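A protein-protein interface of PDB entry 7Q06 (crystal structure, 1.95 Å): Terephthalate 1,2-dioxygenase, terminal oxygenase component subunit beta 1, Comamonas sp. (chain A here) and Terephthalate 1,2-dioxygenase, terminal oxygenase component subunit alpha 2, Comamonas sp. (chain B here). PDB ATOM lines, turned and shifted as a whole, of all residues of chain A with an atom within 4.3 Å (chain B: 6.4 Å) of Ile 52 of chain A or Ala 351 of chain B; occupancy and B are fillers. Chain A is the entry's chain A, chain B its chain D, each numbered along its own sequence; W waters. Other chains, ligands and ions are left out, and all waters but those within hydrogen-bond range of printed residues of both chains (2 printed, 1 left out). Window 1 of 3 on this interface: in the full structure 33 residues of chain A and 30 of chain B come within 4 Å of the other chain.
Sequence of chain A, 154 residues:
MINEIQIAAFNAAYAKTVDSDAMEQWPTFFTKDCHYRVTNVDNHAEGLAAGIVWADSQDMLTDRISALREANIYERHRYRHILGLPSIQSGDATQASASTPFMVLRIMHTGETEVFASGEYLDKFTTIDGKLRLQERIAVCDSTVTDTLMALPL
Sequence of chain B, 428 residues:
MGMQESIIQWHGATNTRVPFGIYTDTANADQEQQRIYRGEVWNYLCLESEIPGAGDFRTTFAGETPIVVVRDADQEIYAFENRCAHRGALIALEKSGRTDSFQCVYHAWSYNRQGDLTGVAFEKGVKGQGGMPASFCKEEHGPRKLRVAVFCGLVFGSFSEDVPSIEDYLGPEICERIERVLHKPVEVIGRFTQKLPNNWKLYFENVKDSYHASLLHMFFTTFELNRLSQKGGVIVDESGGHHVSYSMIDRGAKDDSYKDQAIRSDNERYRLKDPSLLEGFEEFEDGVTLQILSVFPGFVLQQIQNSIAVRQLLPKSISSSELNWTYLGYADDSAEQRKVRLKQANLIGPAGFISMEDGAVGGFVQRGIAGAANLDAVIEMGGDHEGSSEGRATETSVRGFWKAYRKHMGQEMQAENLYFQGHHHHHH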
ATOM      1  N   VAL A  38      25.418  18.806  -8.024  1.00  0.00           N
ATOM      2  CA  VAL A  38      25.566  17.581  -8.843  1.00  0.00           C
ATOM      3  C   VAL A  38      24.279  16.820  -8.676  1.00  0.00           C
ATOM      4  O   VAL A  38      23.953  16.445  -7.522  1.00  0.00           O
ATOM      5  CB  VAL A  38      26.779  16.748  -8.452  1.00  0.00           C
ATOM      6  CG1 VAL A  38      26.792  15.443  -9.225  1.00  0.00           C
ATOM      7  CG2 VAL A  38      28.090  17.513  -8.626  1.00  0.00           C
ATOM      8  N   GLY A  51      21.069  17.792  -4.337  1.00  0.00           N
ATOM      9  CA  GLY A  51      22.299  17.365  -5.014  1.00  0.00           C
ATOM     10  C   GLY A  51      23.113  16.443  -4.127  1.00  0.00           C
ATOM     11  O   GLY A  51      23.067  16.632  -2.887  1.00  0.00           O
ATOM     12  N   ILE A  52      23.893  15.541  -4.738  1.00  0.00           N
ATOM     13  CA  ILE A  52      24.917  14.814  -3.959  1.00  0.00           C
ATOM     14  C   ILE A  52      25.991  15.790  -3.509  1.00  0.00           C
ATOM     15  O   ILE A  52      26.600  15.533  -2.476  1.00  0.00           O
ATOM     16  CB  ILE A  52      25.507  13.618  -4.707  1.00  0.00           C
ATOM     17  CG1 ILE A  52      26.465  13.975  -5.816  1.00  0.00           C
ATOM     18  CG2 ILE A  52      24.463  12.691  -5.226  1.00  0.00           C
ATOM     19  CD1 ILE A  52      27.320  12.808  -6.210  1.00  0.00           C
ATOM     20  N   VAL A  53      26.227  16.857  -4.238  1.00  0.00           N
ATOM     21  CA  VAL A  53      26.892  18.102  -3.750  1.00  0.00           C
ATOM     22  C   VAL A  53      25.870  19.228  -3.948  1.00  0.00           C
ATOM     23  O   VAL A  53      25.241  19.232  -5.022  1.00  0.00           O
ATOM     24  CB  VAL A  53      28.197  18.417  -4.505  1.00  0.00           C
ATOM     25  CG1 VAL A  53      28.812  19.708  -4.013  1.00  0.00           C
ATOM     26  CG2 VAL A  53      29.201  17.296  -4.351  1.00  0.00           C
ATOM     27  N   ARG A  64      34.379  22.218   0.964  1.00  0.00           N
ATOM     28  CA  ARG A  64      34.334  20.859   0.401  1.00  0.00           C
ATOM     29  C   ARG A  64      35.757  20.456   0.044  1.00  0.00           C
ATOM     30  O   ARG A  64      36.150  19.238   0.252  1.00  0.00           O
ATOM     31  CB  ARG A  64      33.307  20.738  -0.730  1.00  0.00           C
ATOM     32  CG  ARG A  64      33.186  19.294  -1.184  1.00  0.00           C
ATOM     33  CD  ARG A  64      31.939  19.042  -1.959  1.00  0.00           C
ATOM     34  NE  ARG A  64      30.789  18.691  -1.147  1.00  0.00           N
ATOM     35  CZ  ARG A  64      30.491  17.459  -0.765  1.00  0.00           C
ATOM     36  NH1 ARG A  64      31.323  16.439  -0.958  1.00  0.00           N
ATOM     37  NH2 ARG A  64      29.355  17.235  -0.113  1.00  0.00           N
ATOM     38  N   THR A 146      26.249   6.474  -8.996  1.00  0.00           N
ATOM     39  CA  THR A 146      27.649   6.821  -8.689  1.00  0.00           C
ATOM     40  C   THR A 146      28.360   5.559  -8.224  1.00  0.00           C
ATOM     41  O   THR A 146      27.845   4.866  -7.279  1.00  0.00           O
ATOM     42  CB  THR A 146      27.736   7.916  -7.636  1.00  0.00           C
ATOM     43  OG1 THR A 146      26.942   9.036  -8.078  1.00  0.00           O
ATOM     44  CG2 THR A 146      29.165   8.282  -7.361  1.00  0.00           C
ATOM     45  N   MET A 150      31.638   9.699  -4.550  1.00  0.00           N
ATOM     46  CA  MET A 150      32.163  10.840  -5.327  1.00  0.00           C
ATOM     47  C   MET A 150      32.893  11.740  -4.343  1.00  0.00           C
ATOM     48  O   MET A 150      32.224  12.258  -3.417  1.00  0.00           O
ATOM     49  CB  MET A 150      31.035  11.604  -6.015  1.00  0.00           C
ATOM     50  CG  MET A 150      31.581  12.705  -6.903  1.00  0.00           C
ATOM     51  SD  MET A 150      30.314  13.642  -7.786  1.00  0.00           S
ATOM     52  CE  MET A 150      29.543  12.324  -8.724  1.00  0.00           C
ATOM     53  N   PHE B 192      19.243   9.181  -5.479  1.00  0.00           N
ATOM     54  CA  PHE B 192      20.607   8.851  -5.953  1.00  0.00           C
ATOM     55  C   PHE B 192      20.909   7.400  -5.629  1.00  0.00           C
ATOM     56  O   PHE B 192      20.557   6.936  -4.523  1.00  0.00           O
ATOM     57  CB  PHE B 192      21.654   9.780  -5.327  1.00  0.00           C
ATOM     58  CG  PHE B 192      21.401  11.243  -5.605  1.00  0.00           C
ATOM     59  CD1 PHE B 192      21.750  11.791  -6.814  1.00  0.00           C
ATOM     60  CD2 PHE B 192      20.779  12.054  -4.656  1.00  0.00           C
ATOM     61  CE1 PHE B 192      21.548  13.145  -7.077  1.00  0.00           C
ATOM     62  CE2 PHE B 192      20.545  13.385  -4.922  1.00  0.00           C
ATOM     63  CZ  PHE B 192      20.935  13.932  -6.137  1.00  0.00           C
ATOM     64  N   GLN B 194      24.050   4.583  -5.221  1.00  0.00           N
ATOM     65  CA  GLN B 194      25.478   4.314  -4.935  1.00  0.00           C
ATOM     66  C   GLN B 194      25.717   2.846  -5.219  1.00  0.00           C
ATOM     67  O   GLN B 194      25.046   2.018  -4.594  1.00  0.00           O
ATOM     68  CB  GLN B 194      25.720   4.644  -3.462  1.00  0.00           C
ATOM     69  CG  GLN B 194      27.061   5.204  -3.152  1.00  0.00           C
ATOM     70  CD  GLN B 194      27.188   5.616  -1.710  1.00  0.00           C
ATOM     71  OE1 GLN B 194      26.227   5.907  -1.002  1.00  0.00           O
ATOM     72  NE2 GLN B 194      28.429   5.725  -1.296  1.00  0.00           N
ATOM     73  N   TYR B 327      15.915  10.859  -0.623  1.00  0.00           N
ATOM     74  CA  TYR B 327      16.086  12.039   0.276  1.00  0.00           C
ATOM     75  C   TYR B 327      14.675  12.600   0.536  1.00  0.00           C
ATOM     76  O   TYR B 327      13.883  12.623  -0.427  1.00  0.00           O
ATOM     77  CB  TYR B 327      16.972  13.144  -0.314  1.00  0.00           C
ATOM     78  CG  TYR B 327      18.448  12.842  -0.503  1.00  0.00           C
ATOM     79  CD1 TYR B 327      19.006  11.577  -0.440  1.00  0.00           C
ATOM     80  CD2 TYR B 327      19.302  13.882  -0.785  1.00  0.00           C
ATOM     81  CE1 TYR B 327      20.369  11.386  -0.623  1.00  0.00           C
ATOM     82  CE2 TYR B 327      20.645  13.697  -0.987  1.00  0.00           C
ATOM     83  CZ  TYR B 327      21.189  12.450  -0.927  1.00  0.00           C
ATOM     84  OH  TYR B 327      22.549  12.365  -1.168  1.00  0.00           O
ATOM     85  N   ALA B 345      22.265  17.755   3.448  1.00  0.00           N
ATOM     86  CA  ALA B 345      22.354  16.562   2.588  1.00  0.00           C
ATOM     87  C   ALA B 345      23.810  16.378   2.129  1.00  0.00           C
ATOM     88  O   ALA B 345      24.145  15.239   1.725  1.00  0.00           O
ATOM     89  CB  ALA B 345      21.422  16.720   1.422  1.00  0.00           C
ATOM     90  N   ASN B 346      24.634  17.439   2.155  1.00  0.00           N
ATOM     91  CA  ASN B 346      26.085  17.314   1.857  1.00  0.00           C
ATOM     92  C   ASN B 346      26.733  16.286   2.790  1.00  0.00           C
ATOM     93  O   ASN B 346      27.849  15.859   2.484  1.00  0.00           O
ATOM     94  CB  ASN B 346      26.837  18.641   1.907  1.00  0.00           C
ATOM     95  CG  ASN B 346      26.540  19.489   0.686  1.00  0.00           C
ATOM     96  OD1 ASN B 346      27.090  19.251  -0.409  1.00  0.00           O
ATOM     97  ND2 ASN B 346      25.656  20.466   0.845  1.00  0.00           N
ATOM     98  N   LEU B 347      26.090  15.949   3.909  1.00  0.00           N
ATOM     99  CA  LEU B 347      26.641  14.977   4.890  1.00  0.00           C
ATOM    100  C   LEU B 347      26.467  13.549   4.399  1.00  0.00           C
ATOM    101  O   LEU B 347      27.243  12.677   4.849  1.00  0.00           O
ATOM    102  CB  LEU B 347      25.939  15.091   6.246  1.00  0.00           C
ATOM    103  CG  LEU B 347      26.160  16.397   6.975  1.00  0.00           C
ATOM    104  CD1 LEU B 347      25.312  16.408   8.233  1.00  0.00           C
ATOM    105  CD2 LEU B 347      27.628  16.607   7.289  1.00  0.00           C
ATOM    106  N   ILE B 348      25.466  13.298   3.550  1.00  0.00           N
ATOM    107  CA  ILE B 348      24.969  11.924   3.241  1.00  0.00           C
ATOM    108  C   ILE B 348      25.094  11.674   1.749  1.00  0.00           C
ATOM    109  O   ILE B 348      25.396  12.584   0.958  1.00  0.00           O
ATOM    110  CB  ILE B 348      23.492  11.789   3.677  1.00  0.00           C
ATOM    111  CG1 ILE B 348      22.565  12.640   2.811  1.00  0.00           C
ATOM    112  CG2 ILE B 348      23.356  12.081   5.168  1.00  0.00           C
ATOM    113  CD1 ILE B 348      21.109  12.247   2.864  1.00  0.00           C
ATOM    114  N   GLY B 349      24.843  10.450   1.377  1.00  0.00           N
ATOM    115  CA  GLY B 349      24.819  10.019  -0.031  1.00  0.00           C
ATOM    116  C   GLY B 349      26.223   9.798  -0.562  1.00  0.00           C
ATOM    117  O   GLY B 349      27.208   9.825   0.157  1.00  0.00           O
ATOM    118  N   PRO B 350      26.328   9.615  -1.876  1.00  0.00           N
ATOM    119  CA  PRO B 350      27.589   9.241  -2.495  1.00  0.00           C
ATOM    120  C   PRO B 350      28.776  10.181  -2.246  1.00  0.00           C
ATOM    121  O   PRO B 350      29.911   9.697  -2.299  1.00  0.00           O
ATOM    122  CB  PRO B 350      27.278   9.223  -3.981  1.00  0.00           C
ATOM    123  CG  PRO B 350      25.784   9.100  -4.063  1.00  0.00           C
ATOM    124  CD  PRO B 350      25.216   9.766  -2.822  1.00  0.00           C
ATOM    125  N   ALA B 351      28.529  11.470  -2.061  1.00  0.00           N
ATOM    126  CA  ALA B 351      29.571  12.506  -1.793  1.00  0.00           C
ATOM    127  C   ALA B 351      29.459  13.017  -0.352  1.00  0.00           C
ATOM    128  O   ALA B 351      29.920  14.103  -0.068  1.00  0.00           O
ATOM    129  CB  ALA B 351      29.490  13.642  -2.757  1.00  0.00           C
ATOM    130  N   GLY B 352      28.831  12.259   0.541  1.00  0.00           N
ATOM    131  CA  GLY B 352      28.573  12.739   1.905  1.00  0.00           C
ATOM    132  C   GLY B 352      29.861  12.888   2.711  1.00  0.00           C
ATOM    133  O   GLY B 352      30.693  11.936   2.697  1.00  0.00           O
ATOM    134  N   PHE B 353      30.018  13.999   3.427  1.00  0.00           N
ATOM    135  CA  PHE B 353      31.123  14.191   4.384  1.00  0.00           C
ATOM    136  C   PHE B 353      31.175  13.006   5.395  1.00  0.00           C
ATOM    137  O   PHE B 353      32.250  12.718   5.905  1.00  0.00           O
ATOM    138  CB  PHE B 353      30.980  15.570   5.030  1.00  0.00           C
ATOM    139  CG  PHE B 353      31.107  16.728   4.063  1.00  0.00           C
ATOM    140  CD1 PHE B 353      32.131  16.776   3.139  1.00  0.00           C
ATOM    141  CD2 PHE B 353      30.209  17.780   4.091  1.00  0.00           C
ATOM    142  CE1 PHE B 353      32.252  17.868   2.267  1.00  0.00           C
ATOM    143  CE2 PHE B 353      30.338  18.880   3.246  1.00  0.00           C
ATOM    144  CZ  PHE B 353      31.359  18.922   2.334  1.00  0.00           C
ATOM    145  N   ILE B 354      30.061  12.319   5.648  1.00  0.00           N
ATOM    146  CA  ILE B 354      30.005  11.029   6.379  1.00  0.00           C
ATOM    147  C   ILE B 354      29.996   9.889   5.369  1.00  0.00           C
ATOM    148  O   ILE B 354      30.868   9.009   5.372  1.00  0.00           O
ATOM    149  CB  ILE B 354      28.714  10.940   7.200  1.00  0.00           C
ATOM    150  CG1 ILE B 354      28.535  12.114   8.165  1.00  0.00           C
ATOM    151  CG2 ILE B 354      28.645   9.585   7.898  1.00  0.00           C
ATOM    152  CD1 ILE B 354      29.771  12.462   8.909  1.00  0.00           C
ATOM    153  N   SER B 355      28.945   9.830   4.583  1.00  0.00           N
ATOM    154  CA  SER B 355      28.527   8.595   3.890  1.00  0.00           C
ATOM    155  C   SER B 355      29.530   8.156   2.812  1.00  0.00           C
ATOM    156  O   SER B 355      29.470   6.985   2.410  1.00  0.00           O
ATOM    157  CB  SER B 355      27.170   8.854   3.287  1.00  0.00           C
ATOM    158  OG  SER B 355      26.223   9.155   4.303  1.00  0.00           O
ATOM    159  N   MET B 356      30.348   9.080   2.280  1.00  0.00           N
ATOM    160  CA  MET B 356      31.287   8.703   1.193  1.00  0.00           C
ATOM    161  C   MET B 356      32.162   7.568   1.739  1.00  0.00           C
ATOM    162  O   MET B 356      32.334   6.628   1.038  1.00  0.00           O
ATOM    163  CB  MET B 356      32.118   9.875   0.630  1.00  0.00           C
ATOM    164  CG  MET B 356      33.284  10.365   1.435  1.00  0.00           C
ATOM    165  SD  MET B 356      34.336  11.432   0.417  1.00  0.00           S
ATOM    166  CE  MET B 356      33.317  12.882   0.205  1.00  0.00           C
HETATM  167  O   HOH W   1      26.190  12.957  -1.641  1.00  0.00           O
HETATM  168  O   HOH W   2      29.303  21.065  -0.552  1.00  0.00           O
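The guanidinium group (NH2) of Arg 64 of chain A is in hydrogen-bond range of the side-chain amide oxygen (OD1) of Asn 346 of chain B (3.0 Å).
The backbone carbonyl oxygen (O) of Ala 351 of chain B lies within hydrogen-bond range of the guanidinium group (NH1) of Arg 64 of chain A (2.9 Å).
O of Pro 350 of chain B is in hydrogen-bond range of N of Met 150 of chain A, at 2.8 Å.
N of Ile 52 of chain A is in hydrogen-bond range of O of Val 38 of chain A (2.9 Å).
The backbone NH of Val 38 of chain A is in hydrogen-bond range of the backbone carbonyl oxygen of Val 53 of chain A (3.0 Å).
O of Asn 346 of chain B is in hydrogen-bond range of N of Phe 353 of chain B (3.0 Å).
The backbone carbonyl oxygen (O) of Leu 347 of chain B sits at hydrogen-bond distance from the backbone NH (N) of Phe 353 of chain B, at 3.4 Å.
Phe 192 of chain B touches Ile 52 of chain A (CD1 to CG2, 3.3 Å).
CD of Pro 350 of chain B touches CG2 of Ile 52 of chain A, at 3.9 Å.
Ile 52 of chain A touches Ala 351 of chain B (O to CB, 3.5 Å).
OD1 of Asn 346 of chain B touches CA of Val 53 of chain A (3.5 Å).
CG2 of Val 53 of chain A touches CB of Ala 351 of chain B, 3.997 Å away.
Arg 64 of chain A touches Phe 353 of chain B.
Gln 194 of chain B touches Thr 146 of chain A (CA to O, 3.4 Å).
CB of Pro 350 of chain B touches CB of Thr 146 of chain A, 3.9 Å away.
Met 150 of chain A touches Ala 351 of chain B.
Met 356 of chain B touches Met 150 of chain A.
Ile 52 of chain A touches just these residues of chain B: Phe 192, Pro 350 and Ala 351.
Printed residues of chain B within 4 Å of Val 53 of chain A: Asn 346 (3.5 Å) and Ala 351 (3.997 Å).
Printed residues of chain B within 4 Å of Arg 64 of chain A: Asn 346, Ala 351 and Phe 353.
Of the printed residues of chain B, Met 150 of chain A touches Pro 350 (2.8 Å), Ala 351 (3.1 Å) and Met 356 (3.8 Å).
Of the printed residues of chain A, Phe 192 of chain B touches Gly 51 and Ile 52.
Of the printed residues of chain A, Asn 346 of chain B touches Val 53 and Arg 64.
Printed residues of chain A within 4 Å of Ala 351 of chain B: Ile 52 (3.5 Å), Val 53 (3.997 Å), Arg 64 (2.9 Å) and Met 150 (3.1 Å).
The nearest residue of chain B that does not touch Ile 52 of chain A is Asn 346 of chain B (4.3 Å).
The nearest printed residue of chain B that does not touch Gly 51 of chain A is Tyr 327 of chain B (4.3 Å).
Of the 15 printed residues of chain B, 7 touch a printed residue of chain A.
Printed residues of chain B that touch a printed residue of chain A: Phe 192, Gln 194, Asn 346, Pro 350, Ala 351, Phe 353 and Met 356.
Of the 7 printed residues of chain A, 6 touch a printed residue of chain B.
Among the printed residues, 14 pairs touch across the chains.
Water W1 lies within hydrogen-bond range of the backbone carbonyl oxygen (O) of Ile 52 of chain A (2.7 Å), the backbone carbonyl oxygen (O) of Ile 348 of chain B (2.7 Å), the backbone NH (N) of Ala 351 of chain B (2.8 Å) and the backbone NH (N) of Gly 352 of chain B (3.5 Å).
Water W2 lies within hydrogen-bond range of NE of Arg 64 of chain A and OD1 of Asn 346 of chain B.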
